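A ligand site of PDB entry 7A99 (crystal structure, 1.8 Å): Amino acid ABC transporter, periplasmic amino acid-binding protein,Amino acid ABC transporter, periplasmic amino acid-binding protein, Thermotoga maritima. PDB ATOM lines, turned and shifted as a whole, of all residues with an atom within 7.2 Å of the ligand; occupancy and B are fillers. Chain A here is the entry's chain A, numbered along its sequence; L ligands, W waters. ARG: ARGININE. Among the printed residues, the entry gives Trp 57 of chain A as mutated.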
ATOM      1  N   LEU A  15      -1.058  -6.963  -8.385  1.00  0.00           N
ATOM      2  CA  LEU A  15      -0.234  -5.777  -8.092  1.00  0.00           C
ATOM      3  C   LEU A  15       1.118  -6.021  -8.725  1.00  0.00           C
ATOM      4  O   LEU A  15       1.415  -7.177  -9.214  1.00  0.00           O
ATOM      5  CB  LEU A  15      -0.146  -5.547  -6.575  1.00  0.00           C
ATOM      6  CG  LEU A  15       0.237  -6.703  -5.642  1.00  0.00           C
ATOM      7  CD1 LEU A  15       1.730  -7.006  -5.729  1.00  0.00           C
ATOM      8  CD2 LEU A  15      -0.186  -6.367  -4.186  1.00  0.00           C
ATOM      9  N   SER A  16       1.928  -4.963  -8.680  1.00  0.00           N
ATOM     10  CA  SER A  16       3.368  -5.010  -9.061  1.00  0.00           C
ATOM     11  C   SER A  16       4.214  -4.691  -7.857  1.00  0.00           C
ATOM     12  O   SER A  16       4.297  -3.551  -7.465  1.00  0.00           O
ATOM     13  CB  SER A  16       3.625  -4.027 -10.187  1.00  0.00           C
ATOM     14  OG  SER A  16       5.022  -3.973 -10.565  1.00  0.00           O
ATOM     15  N   ALA A  17       4.833  -5.735  -7.295  1.00  0.00           N
ATOM     16  CA  ALA A  17       5.519  -5.596  -6.023  1.00  0.00           C
ATOM     17  C   ALA A  17       6.892  -4.899  -6.119  1.00  0.00           C
ATOM     18  O   ALA A  17       7.886  -5.456  -5.663  1.00  0.00           O
ATOM     19  CB  ALA A  17       5.586  -6.933  -5.339  1.00  0.00           C
ATOM     20  N   ASP A  18       6.930  -3.700  -6.678  1.00  0.00           N
ATOM     21  CA  ASP A  18       8.127  -2.883  -6.826  1.00  0.00           C
ATOM     22  C   ASP A  18       7.870  -1.444  -6.408  1.00  0.00           C
ATOM     23  O   ASP A  18       8.412  -0.476  -6.978  1.00  0.00           O
ATOM     24  CB  ASP A  18       8.641  -2.902  -8.292  1.00  0.00           C
ATOM     25  CG  ASP A  18       7.630  -2.295  -9.281  1.00  0.00           C
ATOM     26  OD1 ASP A  18       6.444  -2.035  -8.893  1.00  0.00           O
ATOM     27  OD2 ASP A  18       8.038  -2.081 -10.459  1.00  0.00           O
ATOM     28  N   PHE A  19       7.046  -1.243  -5.378  1.00  0.00           N
ATOM     29  CA  PHE A  19       6.639   0.092  -5.023  1.00  0.00           C
ATOM     30  C   PHE A  19       6.434   0.161  -3.479  1.00  0.00           C
ATOM     31  O   PHE A  19       5.319   0.417  -3.014  1.00  0.00           O
ATOM     32  CB  PHE A  19       5.334   0.425  -5.789  1.00  0.00           C
ATOM     33  CG  PHE A  19       4.912   1.837  -5.756  1.00  0.00           C
ATOM     34  CD1 PHE A  19       5.756   2.891  -6.094  1.00  0.00           C
ATOM     35  CD2 PHE A  19       3.628   2.155  -5.376  1.00  0.00           C
ATOM     36  CE1 PHE A  19       5.304   4.178  -6.104  1.00  0.00           C
ATOM     37  CE2 PHE A  19       3.179   3.473  -5.338  1.00  0.00           C
ATOM     38  CZ  PHE A  19       4.008   4.495  -5.717  1.00  0.00           C
ATOM     39  N   PRO A  20       7.523  -0.047  -2.736  1.00  0.00           N
ATOM     40  CA  PRO A  20       7.414   0.187  -1.273  1.00  0.00           C
ATOM     41  C   PRO A  20       6.974   1.638  -0.979  1.00  0.00           C
ATOM     42  O   PRO A  20       7.320   2.552  -1.713  1.00  0.00           O
ATOM     43  CB  PRO A  20       8.883  -0.079  -0.752  1.00  0.00           C
ATOM     44  CG  PRO A  20       9.733   0.254  -1.942  1.00  0.00           C
ATOM     45  CD  PRO A  20       8.933  -0.218  -3.132  1.00  0.00           C
ATOM     46  N   PHE A  22       3.893   0.474  -0.523  1.00  0.00           N
ATOM     47  CA  PHE A  22       2.553  -0.021  -0.883  1.00  0.00           C
ATOM     48  C   PHE A  22       2.535  -1.479  -1.212  1.00  0.00           C
ATOM     49  O   PHE A  22       1.739  -2.242  -0.640  1.00  0.00           O
ATOM     50  CB  PHE A  22       1.930   0.866  -1.941  1.00  0.00           C
ATOM     51  CG  PHE A  22       1.538   2.147  -1.386  1.00  0.00           C
ATOM     52  CD1 PHE A  22       0.271   2.314  -0.765  1.00  0.00           C
ATOM     53  CD2 PHE A  22       2.451   3.189  -1.320  1.00  0.00           C
ATOM     54  CE1 PHE A  22      -0.030   3.516  -0.172  1.00  0.00           C
ATOM     55  CE2 PHE A  22       2.151   4.375  -0.698  1.00  0.00           C
ATOM     56  CZ  PHE A  22       0.909   4.542  -0.106  1.00  0.00           C
ATOM     57  N   GLU A  23       3.519  -1.916  -2.042  1.00  0.00           N
ATOM     58  CA  GLU A  23       3.759  -3.352  -2.241  1.00  0.00           C
ATOM     59  C   GLU A  23       5.229  -3.564  -2.594  1.00  0.00           C
ATOM     60  O   GLU A  23       5.821  -2.800  -3.368  1.00  0.00           O
ATOM     61  CB  GLU A  23       2.904  -3.911  -3.363  1.00  0.00           C
ATOM     62  CG  GLU A  23       2.821  -3.024  -4.621  1.00  0.00           C
ATOM     63  CD  GLU A  23       1.716  -2.002  -4.509  1.00  0.00           C
ATOM     64  OE1 GLU A  23       0.755  -2.320  -3.751  1.00  0.00           O
ATOM     65  OE2 GLU A  23       1.839  -0.926  -5.071  1.00  0.00           O
ATOM     66  N   ASP A  35      -0.882  -2.067   0.638  1.00  0.00           N
ATOM     67  CA  ASP A  35      -1.854  -2.639  -0.226  1.00  0.00           C
ATOM     68  C   ASP A  35      -2.100  -4.078   0.042  1.00  0.00           C
ATOM     69  O   ASP A  35      -3.205  -4.533  -0.118  1.00  0.00           O
ATOM     70  CB  ASP A  35      -1.444  -2.415  -1.687  1.00  0.00           C
ATOM     71  CG  ASP A  35      -1.602  -0.980  -2.134  1.00  0.00           C
ATOM     72  OD1 ASP A  35      -2.397  -0.200  -1.520  1.00  0.00           O
ATOM     73  OD2 ASP A  35      -1.054  -0.614  -3.221  1.00  0.00           O
ATOM     74  N   MET A  55       2.767  -8.995 -10.864  1.00  0.00           N
ATOM     75  CA  MET A  55       3.072  -8.909 -12.288  1.00  0.00           C
ATOM     76  C   MET A  55       3.701  -7.600 -12.599  1.00  0.00           C
ATOM     77  O   MET A  55       3.774  -6.751 -11.705  1.00  0.00           O
ATOM     78  CB  MET A  55       1.767  -9.156 -13.085  1.00  0.00           C
ATOM     79  CG  MET A  55       0.769  -8.012 -12.981  1.00  0.00           C
ATOM     80  SD  MET A  55      -0.816  -8.501 -13.762  1.00  0.00           S
ATOM     81  CE  MET A  55      -1.453  -9.699 -12.663  1.00  0.00           C
ATOM     82  N   THR A  56       4.146  -7.359 -13.863  1.00  0.00           N
ATOM     83  CA  THR A  56       4.734  -6.048 -14.188  1.00  0.00           C
ATOM     84  C   THR A  56       3.634  -4.988 -14.149  1.00  0.00           C
ATOM     85  O   THR A  56       2.507  -5.371 -14.355  1.00  0.00           O
ATOM     86  CB  THR A  56       5.351  -5.983 -15.617  1.00  0.00           C
ATOM     87  OG1 THR A  56       4.300  -6.077 -16.573  1.00  0.00           O
ATOM     88  CG2 THR A  56       6.356  -7.079 -15.815  1.00  0.00           C
ATOM     89  N   TRP A  57       3.961  -3.730 -13.894  1.00  0.00           N
ATOM     90  CA  TRP A  57       2.971  -2.663 -13.836  1.00  0.00           C
ATOM     91  C   TRP A  57       2.065  -2.650 -15.054  1.00  0.00           C
ATOM     92  O   TRP A  57       0.806  -2.640 -14.950  1.00  0.00           O
ATOM     93  CB  TRP A  57       3.655  -1.313 -13.697  1.00  0.00           C
ATOM     94  CG  TRP A  57       2.754  -0.188 -13.749  1.00  0.00           C
ATOM     95  CD1 TRP A  57       2.618   0.702 -14.765  1.00  0.00           C
ATOM     96  CD2 TRP A  57       1.826   0.172 -12.760  1.00  0.00           C
ATOM     97  NE1 TRP A  57       1.685   1.651 -14.441  1.00  0.00           N
ATOM     98  CE2 TRP A  57       1.193   1.353 -13.202  1.00  0.00           C
ATOM     99  CE3 TRP A  57       1.534  -0.308 -11.487  1.00  0.00           C
ATOM    100  CZ2 TRP A  57       0.187   1.987 -12.465  1.00  0.00           C
ATOM    101  CZ3 TRP A  57       0.530   0.308 -10.750  1.00  0.00           C
ATOM    102  CH2 TRP A  57      -0.125   1.479 -11.254  1.00  0.00           C
ATOM    103  N   LEU A  60      -1.129  -4.991 -15.371  1.00  0.00           N
ATOM    104  CA  LEU A  60      -2.204  -4.996 -14.455  1.00  0.00           C
ATOM    105  C   LEU A  60      -3.619  -4.711 -15.105  1.00  0.00           C
ATOM    106  O   LEU A  60      -4.538  -5.502 -14.891  1.00  0.00           O
ATOM    107  CB  LEU A  60      -1.928  -3.986 -13.352  1.00  0.00           C
ATOM    108  CG  LEU A  60      -0.809  -4.426 -12.393  1.00  0.00           C
ATOM    109  CD1 LEU A  60      -0.362  -3.236 -11.641  1.00  0.00           C
ATOM    110  CD2 LEU A  60      -1.252  -5.593 -11.504  1.00  0.00           C
ATOM    111  N   ILE A  73      -4.893  -3.586  -6.649  1.00  0.00           N
ATOM    112  CA  ILE A  73      -4.520  -2.804  -5.452  1.00  0.00           C
ATOM    113  C   ILE A  73      -2.987  -2.655  -5.475  1.00  0.00           C
ATOM    114  O   ILE A  73      -2.295  -3.508  -5.015  1.00  0.00           O
ATOM    115  CB  ILE A  73      -5.015  -3.445  -4.140  1.00  0.00           C
ATOM    116  CG1 ILE A  73      -6.438  -3.982  -4.270  1.00  0.00           C
ATOM    117  CG2 ILE A  73      -4.813  -2.420  -2.994  1.00  0.00           C
ATOM    118  CD1 ILE A  73      -6.989  -4.588  -3.009  1.00  0.00           C
ATOM    119  N   SER A  74      -2.501  -1.589  -6.091  1.00  0.00           N
ATOM    120  CA  SER A  74      -1.126  -1.507  -6.463  1.00  0.00           C
ATOM    121  C   SER A  74      -0.674  -0.106  -6.557  1.00  0.00           C
ATOM    122  O   SER A  74       0.086   0.246  -7.455  1.00  0.00           O
ATOM    123  CB  SER A  74      -0.934  -2.205  -7.815  1.00  0.00           C
ATOM    124  OG  SER A  74       0.471  -2.376  -8.055  1.00  0.00           O
ATOM    125  N   GLY A  75      -1.056   0.709  -5.569  1.00  0.00           N
ATOM    126  CA  GLY A  75      -0.660   2.124  -5.534  1.00  0.00           C
ATOM    127  C   GLY A  75      -1.111   2.962  -6.748  1.00  0.00           C
ATOM    128  O   GLY A  75      -0.400   3.870  -7.205  1.00  0.00           O
ATOM    129  N   MET A  76      -2.274   2.601  -7.315  1.00  0.00           N
ATOM    130  CA  MET A  76      -2.721   3.208  -8.547  1.00  0.00           C
ATOM    131  C   MET A  76      -3.477   4.521  -8.334  1.00  0.00           C
ATOM    132  O   MET A  76      -4.503   4.565  -7.676  1.00  0.00           O
ATOM    133  CB  MET A  76      -3.593   2.210  -9.351  1.00  0.00           C
ATOM    134  CG  MET A  76      -4.017   2.750 -10.686  1.00  0.00           C
ATOM    135  SD  MET A  76      -4.919   1.506 -11.648  1.00  0.00           S
ATOM    136  CE  MET A  76      -3.600   0.458 -12.229  1.00  0.00           C
ATOM    137  N   THR A  77      -2.961   5.585  -8.915  1.00  0.00           N
ATOM    138  CA  THR A  77      -3.598   6.879  -8.916  1.00  0.00           C
ATOM    139  C   THR A  77      -4.922   6.833  -9.707  1.00  0.00           C
ATOM    140  O   THR A  77      -4.966   6.379 -10.861  1.00  0.00           O
ATOM    141  CB  THR A  77      -2.673   7.924  -9.559  1.00  0.00           C
ATOM    142  OG1 THR A  77      -1.412   7.914  -8.863  1.00  0.00           O
ATOM    143  CG2 THR A  77      -3.263   9.335  -9.587  1.00  0.00           C
ATOM    144  N   ILE A  78      -5.949   7.373  -9.093  1.00  0.00           N
ATOM    145  CA  ILE A  78      -7.251   7.613  -9.750  1.00  0.00           C
ATOM    146  C   ILE A  78      -7.119   8.766 -10.676  1.00  0.00           C
ATOM    147  O   ILE A  78      -6.724   9.821 -10.278  1.00  0.00           O
ATOM    148  CB  ILE A  78      -8.339   7.938  -8.700  1.00  0.00           C
ATOM    149  CG1 ILE A  78      -8.524   6.790  -7.724  1.00  0.00           C
ATOM    150  CG2 ILE A  78      -9.650   8.314  -9.405  1.00  0.00           C
ATOM    151  CD1 ILE A  78      -9.145   7.271  -6.384  1.00  0.00           C
ATOM    152  N   THR A  79      -7.386   8.536 -11.957  1.00  0.00           N
ATOM    153  CA  THR A  79      -7.279   9.584 -12.984  1.00  0.00           C
ATOM    154  C   THR A  79      -8.470   9.439 -13.971  1.00  0.00           C
ATOM    155  O   THR A  79      -9.027   8.345 -14.145  1.00  0.00           O
ATOM    156  CB  THR A  79      -5.981   9.507 -13.836  1.00  0.00           C
ATOM    157  OG1 THR A  79      -5.987   8.325 -14.609  1.00  0.00           O
ATOM    158  CG2 THR A  79      -4.751   9.453 -12.946  1.00  0.00           C
ATOM    159  N   ARG A  82      -7.795   6.948 -16.811  1.00  0.00           N
ATOM    160  CA  ARG A  82      -7.991   5.579 -16.483  1.00  0.00           C
ATOM    161  C   ARG A  82      -9.465   5.194 -16.265  1.00  0.00           C
ATOM    162  O   ARG A  82      -9.807   4.052 -16.483  1.00  0.00           O
ATOM    163  CB  ARG A  82      -7.193   5.191 -15.231  1.00  0.00           C
ATOM    164  CG  ARG A  82      -5.743   4.991 -15.549  1.00  0.00           C
ATOM    165  CD  ARG A  82      -4.878   5.146 -14.295  1.00  0.00           C
ATOM    166  NE  ARG A  82      -3.470   4.967 -14.599  1.00  0.00           N
ATOM    167  CZ  ARG A  82      -2.481   5.100 -13.729  1.00  0.00           C
ATOM    168  NH1 ARG A  82      -2.704   5.463 -12.446  1.00  0.00           N
ATOM    169  NH2 ARG A  82      -1.239   4.867 -14.119  1.00  0.00           N
ATOM    170  N   GLU A 102      -2.055  13.098  -5.674  1.00  0.00           N
ATOM    171  CA  GLU A 102      -2.421  11.792  -6.160  1.00  0.00           C
ATOM    172  C   GLU A 102      -3.300  11.171  -5.049  1.00  0.00           C
ATOM    173  O   GLU A 102      -2.938  11.211  -3.867  1.00  0.00           O
ATOM    174  CB  GLU A 102      -1.175  10.967  -6.453  1.00  0.00           C
ATOM    175  CG  GLU A 102      -0.072  11.715  -7.255  1.00  0.00           C
ATOM    176  CD  GLU A 102      -0.130  11.482  -8.737  1.00  0.00           C
ATOM    177  OE1 GLU A 102      -0.395  10.316  -9.075  1.00  0.00           O
ATOM    178  OE2 GLU A 102       0.123  12.427  -9.556  1.00  0.00           O
ATOM    179  N   GLN A 103      -4.437  10.610  -5.458  1.00  0.00           N
ATOM    180  CA  GLN A 103      -5.207   9.723  -4.605  1.00  0.00           C
ATOM    181  C   GLN A 103      -5.196   8.352  -5.221  1.00  0.00           C
ATOM    182  O   GLN A 103      -5.455   8.213  -6.429  1.00  0.00           O
ATOM    183  CB  GLN A 103      -6.623  10.272  -4.417  1.00  0.00           C
ATOM    184  CG  GLN A 103      -6.664  11.519  -3.554  1.00  0.00           C
ATOM    185  CD  GLN A 103      -8.086  12.047  -3.323  1.00  0.00           C
ATOM    186  OE1 GLN A 103      -8.692  12.535  -4.278  1.00  0.00           O
ATOM    187  NE2 GLN A 103      -8.652  11.907  -2.090  1.00  0.00           N
ATOM    188  N   TYR A 104      -4.893   7.353  -4.415  1.00  0.00           N
ATOM    189  CA  TYR A 104      -4.879   5.991  -4.862  1.00  0.00           C
ATOM    190  C   TYR A 104      -6.224   5.346  -4.677  1.00  0.00           C
ATOM    191  O   TYR A 104      -6.882   5.579  -3.658  1.00  0.00           O
ATOM    192  CB  TYR A 104      -3.839   5.152  -4.167  1.00  0.00           C
ATOM    193  CG  TYR A 104      -2.413   5.617  -4.338  1.00  0.00           C
ATOM    194  CD1 TYR A 104      -2.029   6.562  -5.322  1.00  0.00           C
ATOM    195  CD2 TYR A 104      -1.434   5.089  -3.479  1.00  0.00           C
ATOM    196  CE1 TYR A 104      -0.692   6.948  -5.453  1.00  0.00           C
ATOM    197  CE2 TYR A 104      -0.110   5.492  -3.603  1.00  0.00           C
ATOM    198  CZ  TYR A 104       0.260   6.408  -4.572  1.00  0.00           C
ATOM    199  OH  TYR A 104       1.602   6.771  -4.708  1.00  0.00           O
HETATM  200  N   ARG L   1       0.716   6.079  -8.457  1.00  0.00           N
HETATM  201  CA  ARG L   1       1.436   5.796  -9.786  1.00  0.00           C
HETATM  202  C   ARG L   1       0.470   5.393 -10.878  1.00  0.00           C
HETATM  203  O   ARG L   1      -0.717   5.107 -10.535  1.00  0.00           O
HETATM  204  CB  ARG L   1       2.545   4.722  -9.633  1.00  0.00           C
HETATM  205  CG  ARG L   1       2.115   3.458  -8.988  1.00  0.00           C
HETATM  206  CD  ARG L   1       3.082   2.331  -9.198  1.00  0.00           C
HETATM  207  NE  ARG L   1       2.704   1.121  -8.450  1.00  0.00           N
HETATM  208  CZ  ARG L   1       3.379   0.001  -8.486  1.00  0.00           C
HETATM  209  NH1 ARG L   1       4.463  -0.110  -9.298  1.00  0.00           N
HETATM  210  NH2 ARG L   1       3.006  -1.024  -7.760  1.00  0.00           N
HETATM  211  OXT ARG L   1       0.862   5.241 -12.074  1.00  0.00           O
HETATM  212  O   HOH W   1       5.793   1.641 -11.247  1.00  0.00           O
HETATM  213  O   HOH W   2       3.361   5.202 -13.151  1.00  0.00           O
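N of Gly 75 is in hydrogen-bond range of OE2 of Glu 23 (3.4 Å). The backbone NH (N) of Gly 75 sits at hydrogen-bond distance from the side-chain carboxylate (OD2) of Asp 35 (2.7 Å). The guanidinium group (NH1) of Arg 82 is in hydrogen-bond range of the backbone carbonyl oxygen (O) of Thr 77, at 2.9 Å. OG1 of Thr 79 lies within hydrogen-bond range of N of Arg 82 (3.2 Å). OD1 of Asp 18 sits at hydrogen-bond distance from OG of Ser 16, 2.9 Å away. OG1 of Thr 77 is in hydrogen-bond range of OE1 of Glu 102. The side-chain hydroxyl (OG) of Ser 16 lies close to the backbone carbonyl oxygen (O) of Met 55, at 3.3 Å. The backbone NH (N) of Ser 74 is in hydrogen-bond range of the side-chain carboxylate (OD2) of Asp 35, 3.4 Å away.
Phe 19 touches the ligand (CB to CZ, 3.4 Å). Trp 57 touches the ligand. CA of Met 76 touches O of the ligand, 3.4 Å away. CE1 of Tyr 104 touches N of the ligand, 3.4 Å away. Hydrophobic or aromatic side chains within 4 Å of the ligand: Phe 19, Trp 57 and Tyr 104. Within 4 Å of the ligand: Ser 16, Asp 18, Phe 19, Glu 23, Trp 57, Ser 74, Gly 75, Met 76, Thr 77, Arg 82 and Tyr 104. Along chain A the residues within 4 Å of the ligand span positions 16 to 104. The nearest printed residue that does not touch the ligand is Glu 102 (4.4 Å).
O of Gly 75 is in hydrogen-bond range of N of the ligand (2.8 Å). The guanidinium group (NH1) of Arg 82 is in salt-bridge range of an oxygen (O) of the ligand (2.8 Å). The side-chain carboxylate (OD1) of Asp 18 is in salt-bridge range of a nitrogen (NH1) of the ligand, at 2.8 Å. The backbone NH (N) of Thr 77 is in hydrogen-bond range of an oxygen (O) of the ligand. OG1 of Thr 77 sits at hydrogen-bond distance from N of the ligand (2.8 Å). A nitrogen (NH2) of the ligand lies within hydrogen-bond range of the backbone carbonyl oxygen (O) of Ser 16. The backbone carbonyl oxygen (O) of Ser 74 is in hydrogen-bond range of a nitrogen (NE) of the ligand, at 2.9 Å. NH2 of the ligand sits at hydrogen-bond distance from OG of Ser 74 (2.9 Å). The side-chain carboxylate of Glu 23 lies within salt-bridge range of a nitrogen (NH2) of the ligand (2.9 Å).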
